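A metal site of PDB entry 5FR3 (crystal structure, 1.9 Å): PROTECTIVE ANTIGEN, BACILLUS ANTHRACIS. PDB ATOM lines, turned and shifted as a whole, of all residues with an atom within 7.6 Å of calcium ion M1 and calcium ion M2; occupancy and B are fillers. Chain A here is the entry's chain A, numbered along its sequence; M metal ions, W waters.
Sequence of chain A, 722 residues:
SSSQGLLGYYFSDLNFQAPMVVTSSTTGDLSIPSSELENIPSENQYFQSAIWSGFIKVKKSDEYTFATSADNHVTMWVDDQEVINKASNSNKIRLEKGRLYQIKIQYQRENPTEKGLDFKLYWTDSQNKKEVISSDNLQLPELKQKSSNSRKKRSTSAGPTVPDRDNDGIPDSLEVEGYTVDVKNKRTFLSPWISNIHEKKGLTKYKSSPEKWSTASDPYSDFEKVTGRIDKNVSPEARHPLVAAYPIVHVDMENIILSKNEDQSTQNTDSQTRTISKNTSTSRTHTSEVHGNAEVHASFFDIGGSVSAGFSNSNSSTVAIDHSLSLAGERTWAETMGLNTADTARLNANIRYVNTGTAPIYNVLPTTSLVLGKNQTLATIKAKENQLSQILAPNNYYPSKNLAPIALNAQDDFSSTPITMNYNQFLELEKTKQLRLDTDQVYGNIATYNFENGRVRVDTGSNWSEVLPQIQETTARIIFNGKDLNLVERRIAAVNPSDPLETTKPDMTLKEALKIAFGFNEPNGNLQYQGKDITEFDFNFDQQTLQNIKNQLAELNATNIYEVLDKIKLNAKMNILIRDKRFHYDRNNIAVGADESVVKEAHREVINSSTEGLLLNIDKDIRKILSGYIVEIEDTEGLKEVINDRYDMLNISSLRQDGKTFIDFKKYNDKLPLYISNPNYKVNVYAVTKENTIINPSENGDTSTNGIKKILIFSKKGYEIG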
ATOM      1  N   TYR A   9      10.642 -18.115  34.136  1.00  0.00           N
ATOM      2  CA  TYR A   9      11.661 -19.142  34.308  1.00  0.00           C
ATOM      3  C   TYR A   9      12.218 -18.995  35.716  1.00  0.00           C
ATOM      4  O   TYR A   9      12.748 -17.941  36.055  1.00  0.00           O
ATOM      5  CB  TYR A   9      12.784 -18.947  33.288  1.00  0.00           C
ATOM      6  CG  TYR A   9      12.343 -19.172  31.857  1.00  0.00           C
ATOM      7  CD1 TYR A   9      11.722 -18.163  31.127  1.00  0.00           C
ATOM      8  CD2 TYR A   9      12.548 -20.396  31.227  1.00  0.00           C
ATOM      9  CE1 TYR A   9      11.312 -18.369  29.825  1.00  0.00           C
ATOM     10  CE2 TYR A   9      12.146 -20.601  29.919  1.00  0.00           C
ATOM     11  CZ  TYR A   9      11.528 -19.590  29.226  1.00  0.00           C
ATOM     12  OH  TYR A   9      11.130 -19.791  27.925  1.00  0.00           O
ATOM     13  N   PRO A 163      18.731 -19.674  26.859  1.00  0.00           N
ATOM     14  CA  PRO A 163      19.101 -20.265  25.570  1.00  0.00           C
ATOM     15  C   PRO A 163      17.907 -21.024  25.028  1.00  0.00           C
ATOM     16  O   PRO A 163      17.445 -21.974  25.669  1.00  0.00           O
ATOM     17  CB  PRO A 163      20.235 -21.233  25.937  1.00  0.00           C
ATOM     18  CG  PRO A 163      20.764 -20.740  27.249  1.00  0.00           C
ATOM     19  CD  PRO A 163      19.570 -20.187  27.963  1.00  0.00           C
ATOM     20  N   ASP A 164      17.394 -20.581  23.886  1.00  0.00           N
ATOM     21  CA  ASP A 164      16.206 -21.179  23.288  1.00  0.00           C
ATOM     22  C   ASP A 164      16.320 -20.999  21.781  1.00  0.00           C
ATOM     23  O   ASP A 164      15.591 -20.206  21.181  1.00  0.00           O
ATOM     24  CB  ASP A 164      14.944 -20.515  23.839  1.00  0.00           C
ATOM     25  CG  ASP A 164      13.666 -21.151  23.284  1.00  0.00           C
ATOM     26  OD1 ASP A 164      13.736 -22.255  22.721  1.00  0.00           O
ATOM     27  OD2 ASP A 164      12.592 -20.538  23.425  1.00  0.00           O
ATOM     28  N   ARG A 165      17.224 -21.766  21.188  1.00  0.00           N
ATOM     29  CA  ARG A 165      17.601 -21.608  19.781  1.00  0.00           C
ATOM     30  C   ARG A 165      16.413 -21.672  18.828  1.00  0.00           C
ATOM     31  O   ARG A 165      16.403 -20.986  17.804  1.00  0.00           O
ATOM     32  CB  ARG A 165      18.644 -22.664  19.375  1.00  0.00           C
ATOM     33  CG  ARG A 165      20.014 -22.459  20.002  1.00  0.00           C
ATOM     34  CD  ARG A 165      21.079 -23.330  19.329  1.00  0.00           C
ATOM     35  NE  ARG A 165      20.889 -24.751  19.606  1.00  0.00           N
ATOM     36  CZ  ARG A 165      21.370 -25.371  20.683  1.00  0.00           C
ATOM     37  NH1 ARG A 165      22.063 -24.683  21.584  1.00  0.00           N
ATOM     38  NH2 ARG A 165      21.172 -26.661  20.864  1.00  0.00           N
ATOM     39  N   ASP A 166      15.411 -22.480  19.145  1.00  0.00           N
ATOM     40  CA  ASP A 166      14.300 -22.654  18.215  1.00  0.00           C
ATOM     41  C   ASP A 166      13.055 -21.837  18.573  1.00  0.00           C
ATOM     42  O   ASP A 166      12.047 -21.910  17.877  1.00  0.00           O
ATOM     43  CB  ASP A 166      13.938 -24.148  18.049  1.00  0.00           C
ATOM     44  CG  ASP A 166      13.558 -24.815  19.357  1.00  0.00           C
ATOM     45  OD1 ASP A 166      13.352 -24.109  20.361  1.00  0.00           O
ATOM     46  OD2 ASP A 166      13.428 -26.050  19.367  1.00  0.00           O
ATOM     47  N   ASN A 167      13.138 -21.075  19.653  1.00  0.00           N
ATOM     48  CA  ASN A 167      12.066 -20.164  20.053  1.00  0.00           C
ATOM     49  C   ASN A 167      10.749 -20.847  20.397  1.00  0.00           C
ATOM     50  O   ASN A 167       9.691 -20.232  20.258  1.00  0.00           O
ATOM     51  CB  ASN A 167      11.823 -19.086  18.982  1.00  0.00           C
ATOM     52  CG  ASN A 167      11.265 -17.797  19.565  1.00  0.00           C
ATOM     53  OD1 ASN A 167      11.731 -17.311  20.589  1.00  0.00           O
ATOM     54  ND2 ASN A 167      10.243 -17.241  18.911  1.00  0.00           N
ATOM     55  N   ASP A 168      10.789 -22.104  20.837  1.00  0.00           N
ATOM     56  CA  ASP A 168       9.563 -22.741  21.293  1.00  0.00           C
ATOM     57  C   ASP A 168       9.235 -22.421  22.759  1.00  0.00           C
ATOM     58  O   ASP A 168       8.088 -22.533  23.185  1.00  0.00           O
ATOM     59  CB  ASP A 168       9.529 -24.263  21.010  1.00  0.00           C
ATOM     60  CG  ASP A 168      10.653 -25.035  21.675  1.00  0.00           C
ATOM     61  OD1 ASP A 168      11.338 -24.510  22.595  1.00  0.00           O
ATOM     62  OD2 ASP A 168      10.830 -26.219  21.297  1.00  0.00           O
ATOM     63  N   GLY A 169      10.244 -21.978  23.501  1.00  0.00           N
ATOM     64  CA  GLY A 169      10.038 -21.617  24.900  1.00  0.00           C
ATOM     65  C   GLY A 169      10.769 -22.529  25.875  1.00  0.00           C
ATOM     66  O   GLY A 169      11.013 -22.154  27.023  1.00  0.00           O
ATOM     67  N   ILE A 170      11.091 -23.733  25.421  1.00  0.00           N
ATOM     68  CA  ILE A 170      11.792 -24.693  26.283  1.00  0.00           C
ATOM     69  C   ILE A 170      13.297 -24.467  26.134  1.00  0.00           C
ATOM     70  O   ILE A 170      13.808 -24.453  25.024  1.00  0.00           O
ATOM     71  CB  ILE A 170      11.442 -26.137  25.920  1.00  0.00           C
ATOM     72  CG1 ILE A 170       9.949 -26.297  25.688  1.00  0.00           C
ATOM     73  CG2 ILE A 170      11.923 -27.085  27.007  1.00  0.00           C
ATOM     74  CD1 ILE A 170       9.522 -27.689  25.227  1.00  0.00           C
ATOM     75  N   PRO A 171      14.001 -24.278  27.257  1.00  0.00           N
ATOM     76  CA  PRO A 171      15.448 -24.029  27.203  1.00  0.00           C
ATOM     77  C   PRO A 171      16.182 -25.158  26.489  1.00  0.00           C
ATOM     78  O   PRO A 171      15.733 -26.318  26.583  1.00  0.00           O
ATOM     79  CB  PRO A 171      15.851 -23.979  28.678  1.00  0.00           C
ATOM     80  CG  PRO A 171      14.602 -23.522  29.390  1.00  0.00           C
ATOM     81  CD  PRO A 171      13.473 -24.166  28.630  1.00  0.00           C
ATOM     82  N   ASP A 172      17.270 -24.841  25.773  1.00  0.00           N
ATOM     83  CA  ASP A 172      18.029 -25.841  25.024  1.00  0.00           C
ATOM     84  C   ASP A 172      18.382 -27.049  25.891  1.00  0.00           C
ATOM     85  O   ASP A 172      18.182 -28.198  25.498  1.00  0.00           O
ATOM     86  CB  ASP A 172      19.346 -25.257  24.481  1.00  0.00           C
ATOM     87  CG  ASP A 172      19.135 -24.112  23.512  1.00  0.00           C
ATOM     88  OD1 ASP A 172      18.004 -23.909  23.039  1.00  0.00           O
ATOM     89  OD2 ASP A 172      20.131 -23.419  23.223  1.00  0.00           O
ATOM     90  N   SER A 173      18.915 -26.773  27.082  1.00  0.00           N
ATOM     91  CA  SER A 173      19.409 -27.815  27.973  1.00  0.00           C
ATOM     92  C   SER A 173      18.326 -28.809  28.411  1.00  0.00           C
ATOM     93  O   SER A 173      18.584 -29.999  28.529  1.00  0.00           O
ATOM     94  CB  SER A 173      20.083 -27.194  29.193  1.00  0.00           C
ATOM     95  OG  SER A 173      19.189 -26.345  29.893  1.00  0.00           O
ATOM     96  N   GLU A 175      15.463 -29.586  26.712  1.00  0.00           N
ATOM     97  CA  GLU A 175      15.043 -30.403  25.574  1.00  0.00           C
ATOM     98  C   GLU A 175      16.018 -31.554  25.350  1.00  0.00           C
ATOM     99  O   GLU A 175      15.622 -32.678  25.066  1.00  0.00           O
ATOM    100  CB  GLU A 175      14.923 -29.549  24.304  1.00  0.00           C
ATOM    101  CG  GLU A 175      13.835 -28.485  24.347  1.00  0.00           C
ATOM    102  CD  GLU A 175      13.332 -28.075  22.962  1.00  0.00           C
ATOM    103  OE1 GLU A 175      12.670 -28.903  22.305  1.00  0.00           O
ATOM    104  OE2 GLU A 175      13.571 -26.925  22.550  1.00  0.00           O
ATOM    105  N   TYR A 179      12.911 -33.440  30.154  1.00  0.00           N
ATOM    106  CA  TYR A 179      12.018 -32.602  30.954  1.00  0.00           C
ATOM    107  C   TYR A 179      10.679 -33.280  31.136  1.00  0.00           C
ATOM    108  O   TYR A 179      10.392 -34.305  30.506  1.00  0.00           O
ATOM    109  CB  TYR A 179      11.833 -31.221  30.302  1.00  0.00           C
ATOM    110  CG  TYR A 179      11.276 -31.246  28.892  1.00  0.00           C
ATOM    111  CD1 TYR A 179      12.109 -31.449  27.802  1.00  0.00           C
ATOM    112  CD2 TYR A 179       9.925 -31.031  28.645  1.00  0.00           C
ATOM    113  CE1 TYR A 179      11.612 -31.448  26.509  1.00  0.00           C
ATOM    114  CE2 TYR A 179       9.418 -31.044  27.354  1.00  0.00           C
ATOM    115  CZ  TYR A 179      10.278 -31.248  26.300  1.00  0.00           C
ATOM    116  OH  TYR A 179       9.773 -31.248  25.013  1.00  0.00           O
ATOM    117  N   SER A 208      13.362 -33.535  23.277  1.00  0.00           N
ATOM    118  CA  SER A 208      12.977 -33.000  21.982  1.00  0.00           C
ATOM    119  C   SER A 208      14.170 -32.274  21.391  1.00  0.00           C
ATOM    120  O   SER A 208      15.182 -32.083  22.072  1.00  0.00           O
ATOM    121  CB  SER A 208      11.792 -32.055  22.132  1.00  0.00           C
ATOM    122  OG  SER A 208      12.024 -31.080  23.136  1.00  0.00           O
ATOM    123  N   SER A 209      14.069 -31.877  20.124  1.00  0.00           N
ATOM    124  CA  SER A 209      15.157 -31.122  19.496  1.00  0.00           C
ATOM    125  C   SER A 209      15.129 -29.650  19.891  1.00  0.00           C
ATOM    126  O   SER A 209      14.117 -28.975  19.753  1.00  0.00           O
ATOM    127  CB  SER A 209      15.102 -31.235  17.977  1.00  0.00           C
ATOM    128  OG  SER A 209      16.129 -30.437  17.406  1.00  0.00           O
ATOM    129  N   PRO A 210      16.262 -29.137  20.387  1.00  0.00           N
ATOM    130  CA  PRO A 210      16.364 -27.710  20.716  1.00  0.00           C
ATOM    131  C   PRO A 210      16.499 -26.838  19.474  1.00  0.00           C
ATOM    132  O   PRO A 210      16.593 -25.627  19.596  1.00  0.00           O
ATOM    133  CB  PRO A 210      17.672 -27.641  21.529  1.00  0.00           C
ATOM    134  CG  PRO A 210      18.487 -28.779  21.007  1.00  0.00           C
ATOM    135  CD  PRO A 210      17.490 -29.878  20.774  1.00  0.00           C
ATOM    136  N   GLU A 211      16.518 -27.455  18.295  1.00  0.00           N
ATOM    137  CA  GLU A 211      16.689 -26.738  17.049  1.00  0.00           C
ATOM    138  C   GLU A 211      15.423 -26.791  16.210  1.00  0.00           C
ATOM    139  O   GLU A 211      15.315 -26.121  15.170  1.00  0.00           O
ATOM    140  CB  GLU A 211      17.838 -27.346  16.251  1.00  0.00           C
ATOM    141  CG  GLU A 211      19.072 -27.631  17.073  1.00  0.00           C
ATOM    142  CD  GLU A 211      20.146 -26.615  16.844  1.00  0.00           C
ATOM    143  OE1 GLU A 211      19.807 -25.457  16.545  1.00  0.00           O
ATOM    144  OE2 GLU A 211      21.341 -26.981  16.962  1.00  0.00           O
ATOM    145  N   LYS A 212      14.469 -27.599  16.643  1.00  0.00           N
ATOM    146  CA  LYS A 212      13.203 -27.731  15.930  1.00  0.00           C
ATOM    147  C   LYS A 212      12.064 -27.231  16.795  1.00  0.00           C
ATOM    148  O   LYS A 212      11.801 -27.787  17.853  1.00  0.00           O
ATOM    149  CB  LYS A 212      12.958 -29.200  15.521  1.00  0.00           C
ATOM    150  CG  LYS A 212      13.951 -29.727  14.490  1.00  0.00           C
ATOM    151  CD  LYS A 212      13.706 -31.195  14.148  1.00  0.00           C
ATOM    152  CE  LYS A 212      12.424 -31.376  13.339  1.00  0.00           C
ATOM    153  NZ  LYS A 212      12.532 -30.745  11.997  1.00  0.00           N
ATOM    154  N   TRP A 213      11.416 -26.174  16.337  1.00  0.00           N
ATOM    155  CA  TRP A 213      10.285 -25.581  17.038  1.00  0.00           C
ATOM    156  C   TRP A 213       9.230 -26.651  17.286  1.00  0.00           C
ATOM    157  O   TRP A 213       8.670 -26.774  18.384  1.00  0.00           O
ATOM    158  CB  TRP A 213       9.731 -24.432  16.196  1.00  0.00           C
ATOM    159  CG  TRP A 213       8.495 -23.769  16.715  1.00  0.00           C
ATOM    160  CD1 TRP A 213       8.413 -22.761  17.637  1.00  0.00           C
ATOM    161  CD2 TRP A 213       7.154 -24.037  16.305  1.00  0.00           C
ATOM    162  NE1 TRP A 213       7.103 -22.407  17.832  1.00  0.00           N
ATOM    163  CE2 TRP A 213       6.305 -23.168  17.017  1.00  0.00           C
ATOM    164  CE3 TRP A 213       6.582 -24.943  15.389  1.00  0.00           C
ATOM    165  CZ2 TRP A 213       4.923 -23.180  16.852  1.00  0.00           C
ATOM    166  CZ3 TRP A 213       5.218 -24.945  15.233  1.00  0.00           C
ATOM    167  CH2 TRP A 213       4.399 -24.076  15.951  1.00  0.00           C
ATOM    168  N   SER A 214       8.988 -27.450  16.256  1.00  0.00           N
ATOM    169  CA  SER A 214       8.235 -28.707  16.400  1.00  0.00           C
ATOM    170  C   SER A 214       9.146 -29.859  16.006  1.00  0.00           C
ATOM    171  O   SER A 214       9.528 -29.973  14.841  1.00  0.00           O
ATOM    172  CB  SER A 214       6.986 -28.711  15.523  1.00  0.00           C
ATOM    173  OG  SER A 214       6.385 -30.007  15.530  1.00  0.00           O
ATOM    174  N   THR A 215       9.479 -30.714  16.956  1.00  0.00           N
ATOM    175  CA  THR A 215      10.413 -31.806  16.686  1.00  0.00           C
ATOM    176  C   THR A 215       9.875 -32.811  15.669  1.00  0.00           C
ATOM    177  O   THR A 215      10.631 -33.370  14.886  1.00  0.00           O
ATOM    178  CB  THR A 215      10.848 -32.491  17.979  1.00  0.00           C
ATOM    179  OG1 THR A 215      11.467 -31.506  18.817  1.00  0.00           O
ATOM    180  CG2 THR A 215      11.850 -33.597  17.696  1.00  0.00           C
ATOM    181  N   SER A 221       4.119 -26.548  18.385  1.00  0.00           N
ATOM    182  CA  SER A 221       5.446 -26.476  19.022  1.00  0.00           C
ATOM    183  C   SER A 221       5.607 -27.511  20.139  1.00  0.00           C
ATOM    184  O   SER A 221       4.617 -28.002  20.697  1.00  0.00           O
ATOM    185  CB  SER A 221       5.726 -25.082  19.570  1.00  0.00           C
ATOM    186  OG  SER A 221       5.461 -24.987  20.958  1.00  0.00           O
ATOM    187  N   ASP A 222       6.858 -27.841  20.439  1.00  0.00           N
ATOM    188  CA  ASP A 222       7.139 -28.797  21.509  1.00  0.00           C
ATOM    189  C   ASP A 222       6.560 -28.289  22.827  1.00  0.00           C
ATOM    190  O   ASP A 222       6.055 -29.054  23.635  1.00  0.00           O
ATOM    191  CB  ASP A 222       8.644 -28.985  21.647  1.00  0.00           C
ATOM    192  CG  ASP A 222       9.278 -29.609  20.423  1.00  0.00           C
ATOM    193  OD1 ASP A 222       8.574 -30.316  19.673  1.00  0.00           O
ATOM    194  OD2 ASP A 222      10.496 -29.410  20.220  1.00  0.00           O
ATOM    195  N   PHE A 223       6.630 -26.975  23.015  1.00  0.00           N
ATOM    196  CA  PHE A 223       6.134 -26.330  24.226  1.00  0.00           C
ATOM    197  C   PHE A 223       4.603 -26.301  24.236  1.00  0.00           C
ATOM    198  O   PHE A 223       3.981 -26.579  25.264  1.00  0.00           O
ATOM    199  CB  PHE A 223       6.715 -24.925  24.305  1.00  0.00           C
ATOM    200  CG  PHE A 223       6.255 -24.130  25.500  1.00  0.00           C
ATOM    201  CD1 PHE A 223       6.773 -24.379  26.757  1.00  0.00           C
ATOM    202  CD2 PHE A 223       5.327 -23.110  25.350  1.00  0.00           C
ATOM    203  CE1 PHE A 223       6.356 -23.625  27.852  1.00  0.00           C
ATOM    204  CE2 PHE A 223       4.910 -22.350  26.429  1.00  0.00           C
ATOM    205  CZ  PHE A 223       5.421 -22.622  27.690  1.00  0.00           C
ATOM    206  N   PRO A 241       6.100 -34.601  22.006  1.00  0.00           N
ATOM    207  CA  PRO A 241       6.853 -33.866  20.991  1.00  0.00           C
ATOM    208  C   PRO A 241       7.482 -34.770  19.928  1.00  0.00           C
ATOM    209  O   PRO A 241       7.849 -34.268  18.868  1.00  0.00           O
ATOM    210  CB  PRO A 241       7.952 -33.165  21.819  1.00  0.00           C
ATOM    211  CG  PRO A 241       7.357 -33.028  23.171  1.00  0.00           C
ATOM    212  CD  PRO A 241       6.534 -34.278  23.372  1.00  0.00           C
HETATM  213 CA    CA M   1      13.657 -24.584  22.683  1.00  0.00          CA
HETATM  214 CA    CA M   2      12.225 -27.780  20.210  1.00  0.00          CA
HETATM  215  O   HOH W   1      15.837 -24.786  21.962  1.00  0.00           O
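The backbone NH (N) of Asp 164 sits close to the side-chain carboxylate (OD1) of Asp 172 (3.5 Å).
N of Asp 222 is in hydrogen-bond range of O of Trp 213, at 2.9 Å.
OG of Ser 209 sits close to N of Glu 211, at 3.1 Å.
The backbone NH (N) of Asp 166 sits close to the backbone carbonyl oxygen (O) of Pro 210 (3.4 Å).
The backbone NH (N) of Ser 208 sits at hydrogen-bond distance from the backbone carbonyl oxygen (O) of Glu 175.
OD2 of Asp 164 is in hydrogen-bond range of N of Gly 169 (2.8 Å).
OG1 of Thr 215 sits at hydrogen-bond distance from N of Ser 209, at 2.9 Å.
The side-chain carboxylate (OD1) of Asp 222 lies within hydrogen-bond range of the backbone NH (N) of Thr 215 (2.9 Å).
Of the 26 residues printed, 5 come within 4 Å of calcium ion M1.
The nearest printed residue that does not touch calcium ion M2 is Thr 215 (4.05 Å).
Calcium ion M1 is bound by water W1 (2.3 Å), OD1 of Asp 168 (2.3 Å), OD1 of Asp 164 (2.3 Å), OE2 of Glu 175 (2.3 Å), O of Ile 170 (2.3 Å) and OD1 of Asp 166 (2.4 Å).
OD2 of Asp 166 binds calcium ion M2, at 2.3 Å.
O of Ser 209 binds calcium ion M2, at 2.3 Å.
Calcium ion M2 is bound by OD2 of Asp 168 (2.4 Å).
OD2 of Asp 222 is bound to calcium ion M2.
O of Lys 212 binds calcium ion M2 (2.4 Å).
Calcium ion M2 is bound by the side-chain carboxylate (OE1) of Glu 175, 2.4 Å away.
The side-chain carboxylate (OE2) of Glu 175 binds calcium ion M2, 2.8 Å away.
Calcium ion M2 has seven donor atoms within binding distance.
Water W1 lies within hydrogen-bond range of the side-chain carboxylate of Asp 172 (2.6 Å), the backbone carbonyl oxygen of Pro 210 (2.6 Å) and the backbone NH of Arg 165 (3.4 Å).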
